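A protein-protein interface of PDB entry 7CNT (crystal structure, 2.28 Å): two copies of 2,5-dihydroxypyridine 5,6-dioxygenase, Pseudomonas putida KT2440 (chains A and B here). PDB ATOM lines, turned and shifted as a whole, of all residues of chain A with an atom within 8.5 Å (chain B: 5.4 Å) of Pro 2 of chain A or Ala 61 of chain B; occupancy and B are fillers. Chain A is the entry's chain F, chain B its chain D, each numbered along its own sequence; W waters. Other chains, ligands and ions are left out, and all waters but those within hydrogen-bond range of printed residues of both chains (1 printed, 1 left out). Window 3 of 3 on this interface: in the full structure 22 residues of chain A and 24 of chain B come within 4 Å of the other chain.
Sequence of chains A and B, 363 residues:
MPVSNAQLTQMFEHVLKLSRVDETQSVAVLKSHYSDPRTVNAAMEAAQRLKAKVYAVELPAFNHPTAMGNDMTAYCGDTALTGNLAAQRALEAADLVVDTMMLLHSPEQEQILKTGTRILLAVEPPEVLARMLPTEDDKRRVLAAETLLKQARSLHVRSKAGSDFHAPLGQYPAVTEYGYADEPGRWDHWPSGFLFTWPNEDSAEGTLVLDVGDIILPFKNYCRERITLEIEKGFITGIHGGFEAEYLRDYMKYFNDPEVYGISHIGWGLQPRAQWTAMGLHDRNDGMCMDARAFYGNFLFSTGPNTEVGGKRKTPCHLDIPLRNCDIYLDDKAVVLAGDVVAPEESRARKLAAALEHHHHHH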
ATOM      1  N   PRO A   2     -31.925   9.852 -13.218  1.00  0.00           N
ATOM      2  CA  PRO A   2     -31.176  10.648 -12.265  1.00  0.00           C
ATOM      3  C   PRO A   2     -30.359  11.730 -12.920  1.00  0.00           C
ATOM      4  O   PRO A   2     -30.301  11.793 -14.134  1.00  0.00           O
ATOM      5  CB  PRO A   2     -30.232   9.634 -11.598  1.00  0.00           C
ATOM      6  CG  PRO A   2     -30.912   8.315 -11.729  1.00  0.00           C
ATOM      7  CD  PRO A   2     -31.720   8.405 -13.010  1.00  0.00           C
ATOM      8  N   VAL A   3     -29.679  12.523 -12.087  1.00  0.00           N
ATOM      9  CA  VAL A   3     -29.000  13.748 -12.499  1.00  0.00           C
ATOM     10  C   VAL A   3     -27.511  13.527 -12.820  1.00  0.00           C
ATOM     11  O   VAL A   3     -26.763  13.212 -11.939  1.00  0.00           O
ATOM     12  CB  VAL A   3     -29.063  14.837 -11.393  1.00  0.00           C
ATOM     13  CG1 VAL A   3     -28.560  16.109 -11.944  1.00  0.00           C
ATOM     14  CG2 VAL A   3     -30.453  15.057 -10.868  1.00  0.00           C
ATOM     15  N   SER A   4     -27.085  13.766 -14.068  1.00  0.00           N
ATOM     16  CA  SER A   4     -25.671  13.741 -14.464  1.00  0.00           C
ATOM     17  C   SER A   4     -24.817  14.850 -13.863  1.00  0.00           C
ATOM     18  O   SER A   4     -25.329  15.814 -13.338  1.00  0.00           O
ATOM     19  CB  SER A   4     -25.558  13.863 -15.980  1.00  0.00           C
ATOM     20  OG  SER A   4     -26.046  15.112 -16.435  1.00  0.00           O
ATOM     21  N   ASN A   5     -23.499  14.703 -13.964  1.00  0.00           N
ATOM     22  CA  ASN A   5     -22.557  15.730 -13.526  1.00  0.00           C
ATOM     23  C   ASN A   5     -22.706  17.018 -14.302  1.00  0.00           C
ATOM     24  O   ASN A   5     -22.635  18.097 -13.718  1.00  0.00           O
ATOM     25  CB  ASN A   5     -21.122  15.258 -13.620  1.00  0.00           C
ATOM     26  CG  ASN A   5     -20.786  14.214 -12.566  1.00  0.00           C
ATOM     27  OD1 ASN A   5     -21.670  13.692 -11.882  1.00  0.00           O
ATOM     28  ND2 ASN A   5     -19.503  13.894 -12.438  1.00  0.00           N
ATOM     29  N   ALA A   6     -22.978  16.921 -15.598  1.00  0.00           N
ATOM     30  CA  ALA A   6     -23.186  18.138 -16.382  1.00  0.00           C
ATOM     31  C   ALA A   6     -24.449  18.891 -15.920  1.00  0.00           C
ATOM     32  O   ALA A   6     -24.448  20.094 -15.746  1.00  0.00           O
ATOM     33  CB  ALA A   6     -23.265  17.811 -17.863  1.00  0.00           C
ATOM     34  N   GLN A   7     -25.532  18.177 -15.712  1.00  0.00           N
ATOM     35  CA  GLN A   7     -26.758  18.817 -15.314  1.00  0.00           C
ATOM     36  C   GLN A   7     -26.624  19.376 -13.932  1.00  0.00           C
ATOM     37  O   GLN A   7     -27.109  20.486 -13.689  1.00  0.00           O
ATOM     38  CB  GLN A   7     -27.922  17.854 -15.356  1.00  0.00           C
ATOM     39  CG  GLN A   7     -29.276  18.541 -15.285  1.00  0.00           C
ATOM     40  CD  GLN A   7     -30.430  17.567 -15.417  1.00  0.00           C
ATOM     41  OE1 GLN A   7     -30.284  16.462 -15.945  1.00  0.00           O
ATOM     42  NE2 GLN A   7     -31.577  17.960 -14.915  1.00  0.00           N
ATOM     43  N   LEU A   8     -25.911  18.658 -13.052  1.00  0.00           N
ATOM     44  CA  LEU A   8     -25.714  19.115 -11.672  1.00  0.00           C
ATOM     45  C   LEU A   8     -24.938  20.434 -11.598  1.00  0.00           C
ATOM     46  O   LEU A   8     -25.339  21.345 -10.895  1.00  0.00           O
ATOM     47  CB  LEU A   8     -25.036  18.053 -10.821  1.00  0.00           C
ATOM     48  CG  LEU A   8     -24.978  18.254  -9.313  1.00  0.00           C
ATOM     49  CD1 LEU A   8     -26.322  18.576  -8.697  1.00  0.00           C
ATOM     50  CD2 LEU A   8     -24.427  16.987  -8.662  1.00  0.00           C
ATOM     51  N   MET A  11     -27.189  23.211 -12.926  1.00  0.00           N
ATOM     52  CA  MET A  11     -28.197  23.666 -11.970  1.00  0.00           C
ATOM     53  C   MET A  11     -27.501  24.566 -11.041  1.00  0.00           C
ATOM     54  O   MET A  11     -28.044  25.593 -10.668  1.00  0.00           O
ATOM     55  CB  MET A  11     -28.808  22.517 -11.242  1.00  0.00           C
ATOM     56  CG  MET A  11     -29.805  21.854 -12.181  1.00  0.00           C
ATOM     57  SD  MET A  11     -30.078  19.999 -11.502  1.00  0.00           S
ATOM     58  CE  MET A  11     -29.701  20.136  -9.570  1.00  0.00           C
ATOM     59  N   ARG A  38     -20.247  14.738  -5.232  1.00  0.00           N
ATOM     60  CA  ARG A  38     -20.788  15.273  -6.524  1.00  0.00           C
ATOM     61  C   ARG A  38     -21.390  16.704  -6.401  1.00  0.00           C
ATOM     62  O   ARG A  38     -21.273  17.568  -7.281  1.00  0.00           O
ATOM     63  CB  ARG A  38     -21.855  14.320  -7.047  1.00  0.00           C
ATOM     64  CG  ARG A  38     -21.222  13.004  -7.462  1.00  0.00           C
ATOM     65  CD  ARG A  38     -22.272  12.011  -7.886  1.00  0.00           C
ATOM     66  NE  ARG A  38     -22.748  12.415  -9.196  1.00  0.00           N
ATOM     67  CZ  ARG A  38     -24.005  12.663  -9.523  1.00  0.00           C
ATOM     68  NH1 ARG A  38     -25.010  12.495  -8.651  1.00  0.00           N
ATOM     69  NH2 ARG A  38     -24.247  13.033 -10.787  1.00  0.00           N
ATOM     70  N   PRO A 126     -29.535  15.362  -5.525  1.00  0.00           N
ATOM     71  CA  PRO A 126     -29.628  16.050  -6.815  1.00  0.00           C
ATOM     72  C   PRO A 126     -31.007  15.983  -7.511  1.00  0.00           C
ATOM     73  O   PRO A 126     -31.446  16.980  -8.056  1.00  0.00           O
ATOM     74  CB  PRO A 126     -28.556  15.347  -7.656  1.00  0.00           C
ATOM     75  CG  PRO A 126     -27.532  14.893  -6.672  1.00  0.00           C
ATOM     76  CD  PRO A 126     -28.244  14.652  -5.368  1.00  0.00           C
ATOM     77  N   GLU A 127     -31.707  14.854  -7.452  1.00  0.00           N
ATOM     78  CA  GLU A 127     -33.051  14.751  -8.065  1.00  0.00           C
ATOM     79  C   GLU A 127     -34.061  15.718  -7.421  1.00  0.00           C
ATOM     80  O   GLU A 127     -34.917  16.302  -8.089  1.00  0.00           O
ATOM     81  CB  GLU A 127     -33.585  13.320  -7.995  1.00  0.00           C
ATOM     82  CG  GLU A 127     -32.745  12.378  -8.839  1.00  0.00           C
ATOM     83  CD  GLU A 127     -31.310  12.236  -8.318  1.00  0.00           C
ATOM     84  OE1 GLU A 127     -31.138  12.280  -7.056  1.00  0.00           O
ATOM     85  OE2 GLU A 127     -30.359  12.104  -9.161  1.00  0.00           O
ATOM     86  N   ALA A 130     -33.329  19.271  -8.474  1.00  0.00           N
ATOM     87  CA  ALA A 130     -33.739  19.535  -9.846  1.00  0.00           C
ATOM     88  C   ALA A 130     -35.222  19.739  -9.943  1.00  0.00           C
ATOM     89  O   ALA A 130     -35.689  20.647 -10.625  1.00  0.00           O
ATOM     90  CB  ALA A 130     -33.365  18.361 -10.730  1.00  0.00           C
ATOM     91  N   SER B  32     -23.841   3.903 -16.155  1.00  0.00           N
ATOM     92  CA  SER B  32     -23.758   5.330 -15.925  1.00  0.00           C
ATOM     93  C   SER B  32     -23.244   5.547 -14.503  1.00  0.00           C
ATOM     94  O   SER B  32     -22.800   4.574 -13.854  1.00  0.00           O
ATOM     95  CB  SER B  32     -25.116   5.990 -16.188  1.00  0.00           C
ATOM     96  OG  SER B  32     -25.009   7.405 -16.186  1.00  0.00           O
ATOM     97  N   HIS B  33     -23.267   6.802 -14.033  1.00  0.00           N
ATOM     98  CA  HIS B  33     -22.551   7.210 -12.801  1.00  0.00           C
ATOM     99  C   HIS B  33     -23.091   6.450 -11.621  1.00  0.00           C
ATOM    100  O   HIS B  33     -22.369   6.037 -10.745  1.00  0.00           O
ATOM    101  CB  HIS B  33     -22.580   8.756 -12.557  1.00  0.00           C
ATOM    102  CG  HIS B  33     -23.896   9.266 -12.046  1.00  0.00           C
ATOM    103  ND1 HIS B  33     -24.849   9.834 -12.866  1.00  0.00           N
ATOM    104  CD2 HIS B  33     -24.415   9.284 -10.799  1.00  0.00           C
ATOM    105  CE1 HIS B  33     -25.906  10.160 -12.142  1.00  0.00           C
ATOM    106  NE2 HIS B  33     -25.675   9.822 -10.890  1.00  0.00           N
ATOM    107  N   TYR B  34     -24.377   6.213 -11.644  1.00  0.00           N
ATOM    108  CA  TYR B  34     -25.035   5.536 -10.554  1.00  0.00           C
ATOM    109  C   TYR B  34     -25.028   3.978 -10.645  1.00  0.00           C
ATOM    110  O   TYR B  34     -25.688   3.289  -9.853  1.00  0.00           O
ATOM    111  CB  TYR B  34     -26.470   6.075 -10.492  1.00  0.00           C
ATOM    112  CG  TYR B  34     -27.317   5.824 -11.741  1.00  0.00           C
ATOM    113  CD1 TYR B  34     -27.997   4.598 -11.926  1.00  0.00           C
ATOM    114  CD2 TYR B  34     -27.448   6.819 -12.731  1.00  0.00           C
ATOM    115  CE1 TYR B  34     -28.768   4.382 -13.056  1.00  0.00           C
ATOM    116  CE2 TYR B  34     -28.222   6.623 -13.852  1.00  0.00           C
ATOM    117  CZ  TYR B  34     -28.869   5.415 -14.018  1.00  0.00           C
ATOM    118  OH  TYR B  34     -29.598   5.248 -15.166  1.00  0.00           O
ATOM    119  N   LEU B  59     -22.926   6.231 -20.394  1.00  0.00           N
ATOM    120  CA  LEU B  59     -23.718   7.379 -20.770  1.00  0.00           C
ATOM    121  C   LEU B  59     -23.925   8.310 -19.609  1.00  0.00           C
ATOM    122  O   LEU B  59     -23.981   7.893 -18.455  1.00  0.00           O
ATOM    123  CB  LEU B  59     -25.095   6.973 -21.241  1.00  0.00           C
ATOM    124  CG  LEU B  59     -25.137   6.037 -22.413  1.00  0.00           C
ATOM    125  CD1 LEU B  59     -26.611   5.786 -22.704  1.00  0.00           C
ATOM    126  CD2 LEU B  59     -24.378   6.674 -23.558  1.00  0.00           C
ATOM    127  N   PRO B  60     -24.073   9.587 -19.920  1.00  0.00           N
ATOM    128  CA  PRO B  60     -24.477  10.478 -18.835  1.00  0.00           C
ATOM    129  C   PRO B  60     -25.912  10.164 -18.392  1.00  0.00           C
ATOM    130  O   PRO B  60     -26.746   9.908 -19.214  1.00  0.00           O
ATOM    131  CB  PRO B  60     -24.384  11.879 -19.456  1.00  0.00           C
ATOM    132  CG  PRO B  60     -23.745  11.710 -20.812  1.00  0.00           C
ATOM    133  CD  PRO B  60     -23.769  10.270 -21.190  1.00  0.00           C
ATOM    134  N   ALA B  61     -26.206  10.184 -17.100  1.00  0.00           N
ATOM    135  CA  ALA B  61     -27.608  10.051 -16.651  1.00  0.00           C
ATOM    136  C   ALA B  61     -28.641  10.985 -17.328  1.00  0.00           C
ATOM    137  O   ALA B  61     -28.335  12.077 -17.809  1.00  0.00           O
ATOM    138  CB  ALA B  61     -27.703  10.252 -15.154  1.00  0.00           C
ATOM    139  N   PHE B  62     -29.874  10.502 -17.355  1.00  0.00           N
ATOM    140  CA  PHE B  62     -30.993  11.254 -17.852  1.00  0.00           C
ATOM    141  C   PHE B  62     -31.927  11.494 -16.694  1.00  0.00           C
ATOM    142  O   PHE B  62     -32.325  10.566 -16.019  1.00  0.00           O
ATOM    143  CB  PHE B  62     -31.804  10.528 -18.973  1.00  0.00           C
ATOM    144  CG  PHE B  62     -32.827  11.428 -19.578  1.00  0.00           C
ATOM    145  CD1 PHE B  62     -32.419  12.495 -20.372  1.00  0.00           C
ATOM    146  CD2 PHE B  62     -34.163  11.338 -19.216  1.00  0.00           C
ATOM    147  CE1 PHE B  62     -33.337  13.410 -20.862  1.00  0.00           C
ATOM    148  CE2 PHE B  62     -35.084  12.245 -19.701  1.00  0.00           C
ATOM    149  CZ  PHE B  62     -34.668  13.286 -20.525  1.00  0.00           C
ATOM    150  N   ASN B  63     -32.304  12.746 -16.496  1.00  0.00           N
ATOM    151  CA  ASN B  63     -33.248  13.083 -15.449  1.00  0.00           C
ATOM    152  C   ASN B  63     -34.587  13.643 -15.975  1.00  0.00           C
ATOM    153  O   ASN B  63     -34.605  14.535 -16.810  1.00  0.00           O
ATOM    154  CB  ASN B  63     -32.614  14.078 -14.490  1.00  0.00           C
ATOM    155  CG  ASN B  63     -33.392  14.178 -13.213  1.00  0.00           C
ATOM    156  OD1 ASN B  63     -33.580  13.167 -12.498  1.00  0.00           O
ATOM    157  ND2 ASN B  63     -33.926  15.380 -12.947  1.00  0.00           N
ATOM    158  N   MET B  72     -36.667   4.312 -11.161  1.00  0.00           N
ATOM    159  CA  MET B  72     -36.791   4.885 -12.521  1.00  0.00           C
ATOM    160  C   MET B  72     -37.949   4.332 -13.333  1.00  0.00           C
ATOM    161  O   MET B  72     -38.393   4.994 -14.287  1.00  0.00           O
ATOM    162  CB  MET B  72     -35.494   4.708 -13.311  1.00  0.00           C
ATOM    163  CG  MET B  72     -34.291   5.282 -12.567  1.00  0.00           C
ATOM    164  SD  MET B  72     -32.648   5.004 -13.618  1.00  0.00           S
ATOM    165  CE  MET B  72     -33.266   5.678 -15.366  1.00  0.00           C
ATOM    166  N   ALA B  80     -31.670   8.014 -21.674  1.00  0.00           N
ATOM    167  CA  ALA B  80     -30.320   8.456 -21.989  1.00  0.00           C
ATOM    168  C   ALA B  80     -30.033   8.349 -23.476  1.00  0.00           C
ATOM    169  O   ALA B  80     -29.171   9.054 -23.991  1.00  0.00           O
ATOM    170  CB  ALA B  80     -29.291   7.665 -21.164  1.00  0.00           C
ATOM    171  N   MET B 101     -27.767   0.197 -16.046  1.00  0.00           N
ATOM    172  CA  MET B 101     -28.205   1.562 -15.826  1.00  0.00           C
ATOM    173  C   MET B 101     -29.707   1.721 -15.940  1.00  0.00           C
ATOM    174  O   MET B 101     -30.201   2.822 -15.765  1.00  0.00           O
ATOM    175  CB  MET B 101     -27.447   2.489 -16.759  1.00  0.00           C
ATOM    176  CG  MET B 101     -28.030   2.546 -18.154  1.00  0.00           C
ATOM    177  SD  MET B 101     -27.242   4.088 -19.090  1.00  0.00           S
ATOM    178  CE  MET B 101     -28.405   5.511 -18.382  1.00  0.00           C
HETATM  179  O   HOH W   1     -31.416  15.247 -17.697  1.00  0.00           O
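The backbone NH (N) of Phe 62 of chain B lies close to the backbone carbonyl oxygen (O) of Pro 2 of chain A.
N of Asn 63 of chain B lies within hydrogen-bond range of O of Pro 2 of chain A.
The backbone NH (N) of Ala 61 of chain B lies within hydrogen-bond range of the side-chain hydroxyl (OG) of Ser 32 of chain B, 3.2 Å away.
The side-chain sulfur of Met 72 of chain B sits at hydrogen-bond distance from the side-chain hydroxyl of Tyr 34 of chain B (3.4 Å).
O of Met 101 of chain B lies within hydrogen-bond range of OH of Tyr 34 of chain B.
The backbone carbonyl oxygen of Val 3 of chain A is in hydrogen-bond range of the guanidinium group of Arg 38 of chain A (2.8 Å).
The backbone NH (N) of Val 3 of chain A is in hydrogen-bond range of the side-chain carboxylate (OE2) of Glu 127 of chain A (3.0 Å).
The side-chain hydroxyl (OG) of Ser 4 of chain A lies within hydrogen-bond range of the backbone NH (N) of Gln 7 of chain A, 3.2 Å away.
Pro 2 of chain A touches Tyr 34 of chain B (CG to CE2, 3.8 Å).
Pro 2 of chain A touches Ala 61 of chain B.
CD of Pro 2 of chain A touches SD of Met 72 of chain B, at 3.6 Å.
His 33 of chain B touches Val 3 of chain A (CE1 to O, 3.2 Å).
Val 3 of chain A touches Asn 63 of chain B (CG2 to CG, 3.9 Å).
Ser 4 of chain A touches Ala 61 of chain B.
Asn 63 of chain B touches Gln 7 of chain A (CB to OE1, 3.6 Å).
NH2 of Arg 38 of chain A touches NE2 of His 33 of chain B, 3.5 Å away.
Glu 127 of chain A touches Asn 63 of chain B.
Ala 130 of chain A touches Asn 63 of chain B (CB to ND2, 3.8 Å).
Pro 2 of chain A touches just these residues of chain B: Tyr 34, Ala 61, Phe 62, Asn 63 and Met 72.
Of chain A, only Pro 2 (3.2 Å) and Ser 4 (3.7 Å) come within 4 Å of Ala 61 of chain B.
Printed residues of chain A within 4 Å of Asn 63 of chain B: Pro 2, Val 3, Gln 7, Glu 127 and Ala 130.
Of the printed residues of chain B, Gln 7 of chain A touches Asn 63 (3.6 Å).
Printed residues of chain B within 4 Å of Glu 127 of chain A: Asn 63.
Pro 126 of chain A touches none of the printed residues of chain B.
Ala 6 of chain A touches none of the printed residues of chain B.
The nearest residue of chain A that does not touch Ala 61 of chain B is Val 3 of chain A (4.03 Å).
The nearest printed residue of chain A that does not touch Asn 63 of chain B is Ser 4 of chain A (5.6 Å).
Of the 11 printed residues of chain B, 6 touch a printed residue of chain A.
Of the 12 printed residues of chain A, 7 touch a printed residue of chain B.
Printed residues of chain A that touch a printed residue of chain B: Pro 2, Val 3, Ser 4, Gln 7, Arg 38, Glu 127 and Ala 130.
Hydrophobic or aromatic side chains of chain A that line the printed part of chain B: Pro 2, Val 3 and Ala 130.
Among the printed residues, 12 pairs touch across the chains.
No position is printed for both chains.
Water W1 bridges the side-chain amide oxygen (OE1) of Gln 7 of chain A (2.4 Å) and the backbone NH (N) of Asn 63 of chain B (2.9 Å).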
